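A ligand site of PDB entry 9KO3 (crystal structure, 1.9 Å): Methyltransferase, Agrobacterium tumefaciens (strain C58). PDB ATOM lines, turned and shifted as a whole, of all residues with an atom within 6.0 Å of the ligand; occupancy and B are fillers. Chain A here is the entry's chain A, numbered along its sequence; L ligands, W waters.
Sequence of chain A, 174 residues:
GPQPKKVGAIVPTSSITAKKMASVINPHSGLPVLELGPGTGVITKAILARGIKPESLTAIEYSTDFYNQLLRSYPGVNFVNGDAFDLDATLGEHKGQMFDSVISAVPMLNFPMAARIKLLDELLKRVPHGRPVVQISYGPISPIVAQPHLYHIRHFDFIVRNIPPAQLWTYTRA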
ATOM      1  N   VAL A  11       9.344   5.157 -26.648  1.00  0.00           N
ATOM      2  CA  VAL A  11      10.750   4.823 -26.415  1.00  0.00           C
ATOM      3  C   VAL A  11      11.516   6.097 -26.063  1.00  0.00           C
ATOM      4  O   VAL A  11      11.048   7.199 -26.383  1.00  0.00           O
ATOM      5  CB  VAL A  11      11.377   4.086 -27.607  1.00  0.00           C
ATOM      6  CG1 VAL A  11      10.589   2.817 -27.931  1.00  0.00           C
ATOM      7  CG2 VAL A  11      11.484   4.992 -28.842  1.00  0.00           C
ATOM      8  N   PRO A  12      12.668   6.012 -25.397  1.00  0.00           N
ATOM      9  CA  PRO A  12      13.429   7.225 -25.065  1.00  0.00           C
ATOM     10  C   PRO A  12      13.805   8.036 -26.307  1.00  0.00           C
ATOM     11  O   PRO A  12      14.021   7.508 -27.397  1.00  0.00           O
ATOM     12  CB  PRO A  12      14.674   6.683 -24.369  1.00  0.00           C
ATOM     13  CG  PRO A  12      14.245   5.365 -23.781  1.00  0.00           C
ATOM     14  CD  PRO A  12      13.223   4.805 -24.738  1.00  0.00           C
ATOM     15  N   THR A  13      13.885   9.348 -26.103  1.00  0.00           N
ATOM     16  CA  THR A  13      14.329  10.275 -27.135  1.00  0.00           C
ATOM     17  C   THR A  13      15.745   9.933 -27.586  1.00  0.00           C
ATOM     18  O   THR A  13      16.606   9.581 -26.773  1.00  0.00           O
ATOM     19  CB  THR A  13      14.248  11.697 -26.589  1.00  0.00           C
ATOM     20  OG1 THR A  13      12.882  12.006 -26.301  1.00  0.00           O
ATOM     21  CG2 THR A  13      14.785  12.705 -27.595  1.00  0.00           C
ATOM     22  N   GLU A  35      15.273  21.287 -16.172  1.00  0.00           N
ATOM     23  CA  GLU A  35      14.817  20.201 -17.046  1.00  0.00           C
ATOM     24  C   GLU A  35      13.454  19.709 -16.562  1.00  0.00           C
ATOM     25  O   GLU A  35      13.245  19.540 -15.357  1.00  0.00           O
ATOM     26  CB  GLU A  35      15.825  19.015 -17.088  1.00  0.00           C
ATOM     27  CG  GLU A  35      15.524  18.006 -18.212  1.00  0.00           C
ATOM     28  CD  GLU A  35      16.237  16.640 -18.112  1.00  0.00           C
ATOM     29  OE1 GLU A  35      15.926  15.751 -18.947  1.00  0.00           O
ATOM     30  OE2 GLU A  35      17.118  16.451 -17.243  1.00  0.00           O
ATOM     31  N   LEU A  36      12.514  19.488 -17.484  1.00  0.00           N
ATOM     32  CA  LEU A  36      11.196  18.969 -17.134  1.00  0.00           C
ATOM     33  C   LEU A  36      11.007  17.576 -17.723  1.00  0.00           C
ATOM     34  O   LEU A  36      11.185  17.389 -18.927  1.00  0.00           O
ATOM     35  CB  LEU A  36      10.071  19.902 -17.627  1.00  0.00           C
ATOM     36  CG  LEU A  36      10.216  21.365 -17.265  1.00  0.00           C
ATOM     37  CD1 LEU A  36       9.049  22.151 -17.856  1.00  0.00           C
ATOM     38  CD2 LEU A  36      10.295  21.533 -15.724  1.00  0.00           C
ATOM     39  N   GLY A  37      10.632  16.619 -16.879  1.00  0.00           N
ATOM     40  CA  GLY A  37      10.330  15.271 -17.307  1.00  0.00           C
ATOM     41  C   GLY A  37      11.525  14.451 -17.787  1.00  0.00           C
ATOM     42  O   GLY A  37      11.543  13.983 -18.926  1.00  0.00           O
ATOM     43  N   PRO A  38      12.519  14.230 -16.916  1.00  0.00           N
ATOM     44  CA  PRO A  38      13.786  13.577 -17.351  1.00  0.00           C
ATOM     45  C   PRO A  38      13.684  12.079 -17.701  1.00  0.00           C
ATOM     46  O   PRO A  38      14.539  11.593 -18.459  1.00  0.00           O
ATOM     47  CB  PRO A  38      14.723  13.789 -16.159  1.00  0.00           C
ATOM     48  CG  PRO A  38      13.792  13.974 -14.977  1.00  0.00           C
ATOM     49  CD  PRO A  38      12.603  14.704 -15.515  1.00  0.00           C
ATOM     50  N   GLY A  39      12.728  11.337 -17.165  1.00  0.00           N
ATOM     51  CA  GLY A  39      12.528   9.964 -17.631  1.00  0.00           C
ATOM     52  C   GLY A  39      13.728   9.074 -17.341  1.00  0.00           C
ATOM     53  O   GLY A  39      14.193   8.984 -16.203  1.00  0.00           O
ATOM     54  N   THR A  40      14.244   8.405 -18.382  1.00  0.00           N
ATOM     55  CA  THR A  40      15.452   7.586 -18.244  1.00  0.00           C
ATOM     56  C   THR A  40      16.724   8.415 -18.106  1.00  0.00           C
ATOM     57  O   THR A  40      17.761   7.854 -17.763  1.00  0.00           O
ATOM     58  CB  THR A  40      15.625   6.638 -19.436  1.00  0.00           C
ATOM     59  OG1 THR A  40      15.771   7.401 -20.652  1.00  0.00           O
ATOM     60  CG2 THR A  40      14.455   5.659 -19.538  1.00  0.00           C
ATOM     61  N   GLY A  41      16.667   9.713 -18.389  1.00  0.00           N
ATOM     62  CA  GLY A  41      17.831  10.555 -18.223  1.00  0.00           C
ATOM     63  C   GLY A  41      18.631  10.849 -19.466  1.00  0.00           C
ATOM     64  O   GLY A  41      19.733  11.396 -19.354  1.00  0.00           O
ATOM     65  N   VAL A  42      18.124  10.527 -20.657  1.00  0.00           N
ATOM     66  CA  VAL A  42      18.922  10.738 -21.865  1.00  0.00           C
ATOM     67  C   VAL A  42      19.133  12.239 -22.131  1.00  0.00           C
ATOM     68  O   VAL A  42      20.198  12.649 -22.611  1.00  0.00           O
ATOM     69  CB  VAL A  42      18.283  10.029 -23.078  1.00  0.00           C
ATOM     70  CG1 VAL A  42      16.835  10.489 -23.307  1.00  0.00           C
ATOM     71  CG2 VAL A  42      19.119  10.272 -24.331  1.00  0.00           C
ATOM     72  N   ILE A  43      18.156  13.084 -21.821  1.00  0.00           N
ATOM     73  CA  ILE A  43      18.423  14.507 -22.018  1.00  0.00           C
ATOM     74  C   ILE A  43      19.286  15.049 -20.881  1.00  0.00           C
ATOM     75  O   ILE A  43      20.157  15.900 -21.116  1.00  0.00           O
ATOM     76  CB  ILE A  43      17.115  15.304 -22.191  1.00  0.00           C
ATOM     77  CG1 ILE A  43      16.316  14.756 -23.373  1.00  0.00           C
ATOM     78  CG2 ILE A  43      17.405  16.782 -22.442  1.00  0.00           C
ATOM     79  CD1 ILE A  43      15.053  15.525 -23.680  1.00  0.00           C
ATOM     80  N   ILE A  60      12.590  18.043 -12.804  1.00  0.00           N
ATOM     81  CA  ILE A  60      11.308  17.765 -12.149  1.00  0.00           C
ATOM     82  C   ILE A  60      10.674  16.568 -12.835  1.00  0.00           C
ATOM     83  O   ILE A  60      10.390  16.607 -14.034  1.00  0.00           O
ATOM     84  CB  ILE A  60      10.367  18.979 -12.196  1.00  0.00           C
ATOM     85  CG1 ILE A  60      11.028  20.202 -11.560  1.00  0.00           C
ATOM     86  CG2 ILE A  60       9.035  18.653 -11.528  1.00  0.00           C
ATOM     87  CD1 ILE A  60      10.208  21.541 -11.715  1.00  0.00           C
ATOM     88  N   GLU A  61      10.422  15.495 -12.062  1.00  0.00           N
ATOM     89  CA  GLU A  61       9.924  14.219 -12.575  1.00  0.00           C
ATOM     90  C   GLU A  61       8.746  13.741 -11.735  1.00  0.00           C
ATOM     91  O   GLU A  61       8.880  13.591 -10.517  1.00  0.00           O
ATOM     92  CB  GLU A  61      11.049  13.174 -12.571  1.00  0.00           C
ATOM     93  CG  GLU A  61      10.624  11.751 -12.942  1.00  0.00           C
ATOM     94  CD  GLU A  61       9.834  11.689 -14.230  1.00  0.00           C
ATOM     95  OE1 GLU A  61       8.655  11.273 -14.202  1.00  0.00           O
ATOM     96  OE2 GLU A  61      10.386  12.079 -15.283  1.00  0.00           O
ATOM     97  N   TYR A  62       7.604  13.500 -12.375  1.00  0.00           N
ATOM     98  CA  TYR A  62       6.436  13.061 -11.621  1.00  0.00           C
ATOM     99  C   TYR A  62       6.576  11.604 -11.169  1.00  0.00           C
ATOM    100  O   TYR A  62       6.255  11.288 -10.015  1.00  0.00           O
ATOM    101  CB  TYR A  62       5.147  13.236 -12.434  1.00  0.00           C
ATOM    102  CG  TYR A  62       3.895  13.038 -11.599  1.00  0.00           C
ATOM    103  CD1 TYR A  62       3.344  14.083 -10.878  1.00  0.00           C
ATOM    104  CD2 TYR A  62       3.279  11.790 -11.508  1.00  0.00           C
ATOM    105  CE1 TYR A  62       2.199  13.910 -10.087  1.00  0.00           C
ATOM    106  CE2 TYR A  62       2.143  11.589 -10.729  1.00  0.00           C
ATOM    107  CZ  TYR A  62       1.601  12.664 -10.021  1.00  0.00           C
ATOM    108  OH  TYR A  62       0.486  12.503  -9.236  1.00  0.00           O
ATOM    109  N   SER A  63       7.059  10.714 -12.035  1.00  0.00           N
ATOM    110  CA  SER A  63       7.087   9.291 -11.708  1.00  0.00           C
ATOM    111  C   SER A  63       8.077   9.042 -10.581  1.00  0.00           C
ATOM    112  O   SER A  63       9.270   9.348 -10.702  1.00  0.00           O
ATOM    113  CB  SER A  63       7.464   8.467 -12.942  1.00  0.00           C
ATOM    114  OG  SER A  63       7.919   7.167 -12.578  1.00  0.00           O
ATOM    115  N   PHE A  66      10.795   6.452 -11.820  1.00  0.00           N
ATOM    116  CA  PHE A  66      11.867   7.112 -12.563  1.00  0.00           C
ATOM    117  C   PHE A  66      12.747   7.960 -11.635  1.00  0.00           C
ATOM    118  O   PHE A  66      13.982   7.947 -11.749  1.00  0.00           O
ATOM    119  CB  PHE A  66      11.277   8.008 -13.652  1.00  0.00           C
ATOM    120  CG  PHE A  66      10.915   7.291 -14.922  1.00  0.00           C
ATOM    121  CD1 PHE A  66      11.648   6.175 -15.352  1.00  0.00           C
ATOM    122  CD2 PHE A  66       9.854   7.741 -15.701  1.00  0.00           C
ATOM    123  CE1 PHE A  66      11.315   5.522 -16.543  1.00  0.00           C
ATOM    124  CE2 PHE A  66       9.515   7.096 -16.888  1.00  0.00           C
ATOM    125  CZ  PHE A  66      10.248   5.980 -17.317  1.00  0.00           C
ATOM    126  N   GLY A  82       7.797  15.594  -8.453  1.00  0.00           N
ATOM    127  CA  GLY A  82       6.553  16.342  -8.408  1.00  0.00           C
ATOM    128  C   GLY A  82       6.058  16.726  -9.787  1.00  0.00           C
ATOM    129  O   GLY A  82       6.539  16.252 -10.815  1.00  0.00           O
ATOM    130  N   ASP A  83       5.064  17.608  -9.789  1.00  0.00           N
ATOM    131  CA  ASP A  83       4.342  18.003 -10.998  1.00  0.00           C
ATOM    132  C   ASP A  83       4.903  19.315 -11.518  1.00  0.00           C
ATOM    133  O   ASP A  83       4.816  20.346 -10.836  1.00  0.00           O
ATOM    134  CB  ASP A  83       2.839  18.130 -10.701  1.00  0.00           C
ATOM    135  CG  ASP A  83       2.014  18.542 -11.922  1.00  0.00           C
ATOM    136  OD1 ASP A  83       2.531  18.582 -13.069  1.00  0.00           O
ATOM    137  OD2 ASP A  83       0.820  18.813 -11.723  1.00  0.00           O
ATOM    138  N   ALA A  84       5.460  19.289 -12.731  1.00  0.00           N
ATOM    139  CA  ALA A  84       6.046  20.482 -13.340  1.00  0.00           C
ATOM    140  C   ALA A  84       5.026  21.575 -13.603  1.00  0.00           C
ATOM    141  O   ALA A  84       5.415  22.747 -13.725  1.00  0.00           O
ATOM    142  CB  ALA A  84       6.747  20.108 -14.659  1.00  0.00           C
ATOM    143  N   PHE A  85       3.741  21.257 -13.704  1.00  0.00           N
ATOM    144  CA  PHE A  85       2.732  22.296 -13.838  1.00  0.00           C
ATOM    145  C   PHE A  85       2.450  23.013 -12.518  1.00  0.00           C
ATOM    146  O   PHE A  85       1.746  24.028 -12.521  1.00  0.00           O
ATOM    147  CB  PHE A  85       1.445  21.715 -14.420  1.00  0.00           C
ATOM    148  CG  PHE A  85       1.545  21.356 -15.888  1.00  0.00           C
ATOM    149  CD1 PHE A  85       2.223  20.205 -16.287  1.00  0.00           C
ATOM    150  CD2 PHE A  85       0.964  22.170 -16.852  1.00  0.00           C
ATOM    151  CE1 PHE A  85       2.332  19.888 -17.642  1.00  0.00           C
ATOM    152  CE2 PHE A  85       1.061  21.853 -18.199  1.00  0.00           C
ATOM    153  CZ  PHE A  85       1.739  20.702 -18.598  1.00  0.00           C
ATOM    154  N   ALA A 105      10.598  18.048 -21.837  1.00  0.00           N
ATOM    155  CA  ALA A 105      10.072  16.896 -22.551  1.00  0.00           C
ATOM    156  C   ALA A 105       8.785  16.361 -21.907  1.00  0.00           C
ATOM    157  O   ALA A 105       8.417  15.201 -22.142  1.00  0.00           O
ATOM    158  CB  ALA A 105      11.135  15.801 -22.663  1.00  0.00           C
ATOM    159  N   VAL A 106       8.075  17.177 -21.134  1.00  0.00           N
ATOM    160  CA  VAL A 106       6.768  16.723 -20.644  1.00  0.00           C
ATOM    161  C   VAL A 106       5.838  16.532 -21.838  1.00  0.00           C
ATOM    162  O   VAL A 106       5.930  17.289 -22.821  1.00  0.00           O
ATOM    163  CB  VAL A 106       6.155  17.680 -19.603  1.00  0.00           C
ATOM    164  CG1 VAL A 106       6.945  17.598 -18.317  1.00  0.00           C
ATOM    165  CG2 VAL A 106       6.054  19.105 -20.112  1.00  0.00           C
ATOM    166  N   PRO A 107       4.964  15.508 -21.808  1.00  0.00           N
ATOM    167  CA  PRO A 107       4.064  15.262 -22.934  1.00  0.00           C
ATOM    168  C   PRO A 107       2.893  16.236 -22.969  1.00  0.00           C
ATOM    169  O   PRO A 107       1.798  15.959 -22.443  1.00  0.00           O
ATOM    170  CB  PRO A 107       3.620  13.810 -22.720  1.00  0.00           C
ATOM    171  CG  PRO A 107       3.687  13.633 -21.214  1.00  0.00           C
ATOM    172  CD  PRO A 107       4.810  14.507 -20.731  1.00  0.00           C
ATOM    173  N   PHE A 111      -2.223  17.209 -21.728  1.00  0.00           N
ATOM    174  CA  PHE A 111      -2.822  18.241 -20.878  1.00  0.00           C
ATOM    175  C   PHE A 111      -3.645  19.222 -21.705  1.00  0.00           C
ATOM    176  O   PHE A 111      -3.377  19.399 -22.899  1.00  0.00           O
ATOM    177  CB  PHE A 111      -1.722  19.006 -20.106  1.00  0.00           C
ATOM    178  CG  PHE A 111      -0.781  18.116 -19.344  1.00  0.00           C
ATOM    179  CD1 PHE A 111       0.368  17.626 -19.949  1.00  0.00           C
ATOM    180  CD2 PHE A 111      -1.029  17.783 -18.009  1.00  0.00           C
ATOM    181  CE1 PHE A 111       1.245  16.791 -19.229  1.00  0.00           C
ATOM    182  CE2 PHE A 111      -0.157  16.949 -17.298  1.00  0.00           C
ATOM    183  CZ  PHE A 111       0.986  16.460 -17.911  1.00  0.00           C
ATOM    184  N   ILE A 136      10.030  19.463 -26.971  1.00  0.00           N
ATOM    185  CA  ILE A 136       9.922  18.423 -27.988  1.00  0.00           C
ATOM    186  C   ILE A 136       8.450  18.087 -28.198  1.00  0.00           C
ATOM    187  O   ILE A 136       7.663  18.045 -27.234  1.00  0.00           O
ATOM    188  CB  ILE A 136      10.747  17.165 -27.599  1.00  0.00           C
ATOM    189  CG1 ILE A 136      10.666  16.097 -28.689  1.00  0.00           C
ATOM    190  CG2 ILE A 136      10.264  16.602 -26.271  1.00  0.00           C
ATOM    191  CD1 ILE A 136      11.775  15.020 -28.596  1.00  0.00           C
ATOM    192  N   TYR A 138       5.633  16.045 -31.509  1.00  0.00           N
ATOM    193  CA  TYR A 138       5.615  15.104 -32.630  1.00  0.00           C
ATOM    194  C   TYR A 138       4.634  15.456 -33.730  1.00  0.00           C
ATOM    195  O   TYR A 138       4.756  14.909 -34.832  1.00  0.00           O
ATOM    196  CB  TYR A 138       5.323  13.676 -32.109  1.00  0.00           C
ATOM    197  CG  TYR A 138       6.267  13.310 -30.986  1.00  0.00           C
ATOM    198  CD1 TYR A 138       7.575  12.937 -31.247  1.00  0.00           C
ATOM    199  CD2 TYR A 138       5.878  13.404 -29.654  1.00  0.00           C
ATOM    200  CE1 TYR A 138       8.463  12.639 -30.219  1.00  0.00           C
ATOM    201  CE2 TYR A 138       6.749  13.113 -28.614  1.00  0.00           C
ATOM    202  CZ  TYR A 138       8.050  12.731 -28.908  1.00  0.00           C
ATOM    203  OH  TYR A 138       8.943  12.427 -27.886  1.00  0.00           O
HETATM  204  N1  LIG L   1      13.075  13.083 -21.276  1.00  0.00           N
HETATM  205  C1  LIG L   1      12.783  11.671 -21.503  1.00  0.00           C
HETATM  206  C2  LIG L   1      11.371  11.281 -21.051  1.00  0.00           C
HETATM  207  C3  LIG L   1      10.275  11.847 -21.968  1.00  0.00           C
HETATM  208  S1  LIG L   1       8.652  11.092 -21.591  1.00  0.00           S
HETATM  209  C4  LIG L   1      12.978  11.400 -22.994  1.00  0.00           C
HETATM  210  O1  LIG L   1      13.013  12.380 -23.784  1.00  0.00           O
HETATM  211  O2  LIG L   1      13.121  10.223 -23.436  1.00  0.00           O
HETATM  212  C5  LIG L   1       7.817  12.291 -20.496  1.00  0.00           C
HETATM  213  C6  LIG L   1       8.405  12.306 -19.053  1.00  0.00           C
HETATM  214  O3  LIG L   1       7.820  13.281 -18.372  1.00  0.00           O
HETATM  215  C7  LIG L   1       8.064  11.012 -18.288  1.00  0.00           C
HETATM  216  O4  LIG L   1       9.157  10.584 -17.587  1.00  0.00           O
HETATM  217  C8  LIG L   1       6.914  11.450 -17.348  1.00  0.00           C
HETATM  218  O5  LIG L   1       6.876  10.604 -16.124  1.00  0.00           O
HETATM  219  C9  LIG L   1       7.212  12.689 -17.013  1.00  0.00           C
HETATM  220  N2  LIG L   1       6.095  13.577 -16.770  1.00  0.00           N
HETATM  221  C10 LIG L   1       4.926  13.608 -17.398  1.00  0.00           C
HETATM  222  N3  LIG L   1       4.194  14.613 -16.892  1.00  0.00           N
HETATM  223  C11 LIG L   1       4.933  15.237 -15.961  1.00  0.00           C
HETATM  224  C12 LIG L   1       4.670  16.325 -15.159  1.00  0.00           C
HETATM  225  N4  LIG L   1       3.466  17.136 -15.081  1.00  0.00           N
HETATM  226  N5  LIG L   1       5.577  16.756 -14.284  1.00  0.00           N
HETATM  227  C13 LIG L   1       6.773  16.137 -14.196  1.00  0.00           C
HETATM  228  N6  LIG L   1       7.032  15.070 -14.991  1.00  0.00           N
HETATM  229  C14 LIG L   1       6.112  14.615 -15.887  1.00  0.00           C
HETATM  230  O   HOH W   1       4.110  10.701 -15.480  1.00  0.00           O
HETATM  231  O   HOH W   2      16.000  13.167 -19.952  1.00  0.00           O
HETATM  232  O   HOH W   3       3.056  10.829 -18.137  1.00  0.00           O
HETATM  233  O   HOH W   4      13.441   8.522 -21.324  1.00  0.00           O
HETATM  234  O   HOH W   5      13.656  16.188 -20.312  1.00  0.00           O
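Residues that only touch the ligand: Pro 12 (3.4 Å), Pro 38 (3.5 Å), Gly 39 (3.4 Å), Val 42 (3.7 Å), Ile 43 (3.8 Å), Ile 60 (3.7 Å), Ser 63 (3.9 Å), Phe 66 (3.5 Å), Gly 82 (3.4 Å), Phe 85 (3.5 Å), Ala 105 (3.4 Å), Val 106 (3.9 Å), Pro 107 (3.5 Å) and Phe 111 (3.8 Å). Hydrophobic or aromatic side chains that line the ligand: Pro 12, Val 42, Ile 43, Tyr 62, Phe 66, Ala 84, Phe 85, Ala 105, Val 106, Pro 107 and Phe 111. Within 4 Å of the ligand: Pro 12, Thr 13, Gly 37, Pro 38, Gly 39, Val 42, Ile 43, Ile 60, Glu 61, Tyr 62, Ser 63, Phe 66, Gly 82, Asp 83, Ala 84, Phe 85, Ala 105, Val 106, Pro 107 and Phe 111. The nearest printed residue that does not touch the ligand is Glu 35 (4.5 Å).
The backbone NH of Tyr 62 lies within hydrogen-bond range of a nitrogen (N6) of the ligand, at 3.1 Å. The backbone NH of Ala 84 lies within hydrogen-bond range of a nitrogen (N5) of the ligand, 3.0 Å away. OG1 of Thr 13 lies within hydrogen-bond range of O1 of the ligand. The backbone NH (N) of Thr 13 sits at hydrogen-bond distance from an oxygen (O2) of the ligand (2.9 Å). The backbone carbonyl oxygen of Gly 37 lies within hydrogen-bond range of a nitrogen (N1) of the ligand, 2.9 Å away. An oxygen (O5) of the ligand lies within hydrogen-bond range of the side-chain carboxylate (OE1) of Glu 61 (2.7 Å). A nitrogen (N4) of the ligand is in hydrogen-bond range of the side-chain carboxylate (OD1) of Asp 83 (2.6 Å).
The side-chain hydroxyl of Ser 63 is in hydrogen-bond range of the backbone NH of Phe 66. The backbone NH of Ala 105 lies within hydrogen-bond range of the backbone carbonyl oxygen of Leu 36, at 3.0 Å. The backbone NH (N) of Ser 63 sits at hydrogen-bond distance from the side-chain carboxylate (OE1) of Glu 61 (2.7 Å). The backbone NH (N) of Ile 60 sits at hydrogen-bond distance from the backbone carbonyl oxygen (O) of Glu 35 (3.0 Å). The backbone carbonyl oxygen (O) of Ile 60 sits at hydrogen-bond distance from the backbone NH (N) of Gly 37 (2.9 Å). The side-chain carboxylate (OE2) of Glu 61 is in hydrogen-bond range of the backbone NH (N) of Gly 39, 3.1 Å away. The backbone carbonyl oxygen (O) of Glu 61 is in hydrogen-bond range of the backbone NH (N) of Gly 82, 3.1 Å away. The backbone NH (N) of Tyr 62 lies close to the backbone carbonyl oxygen (O) of Gly 82.
Water W4 bridges the side-chain hydroxyl (OG1) of Thr 40 (2.7 Å) and an oxygen (O2) of the ligand (2.7 Å). Water W2 lies within hydrogen-bond range of the backbone carbonyl oxygen of Pro 38 (2.6 Å), the side-chain carboxylate of Glu 35 (2.8 Å), the backbone NH of Ile 43 (2.9 Å), a nitrogen (N1) of the ligand (3.2 Å) and the backbone NH of Val 42 (3.5 Å).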
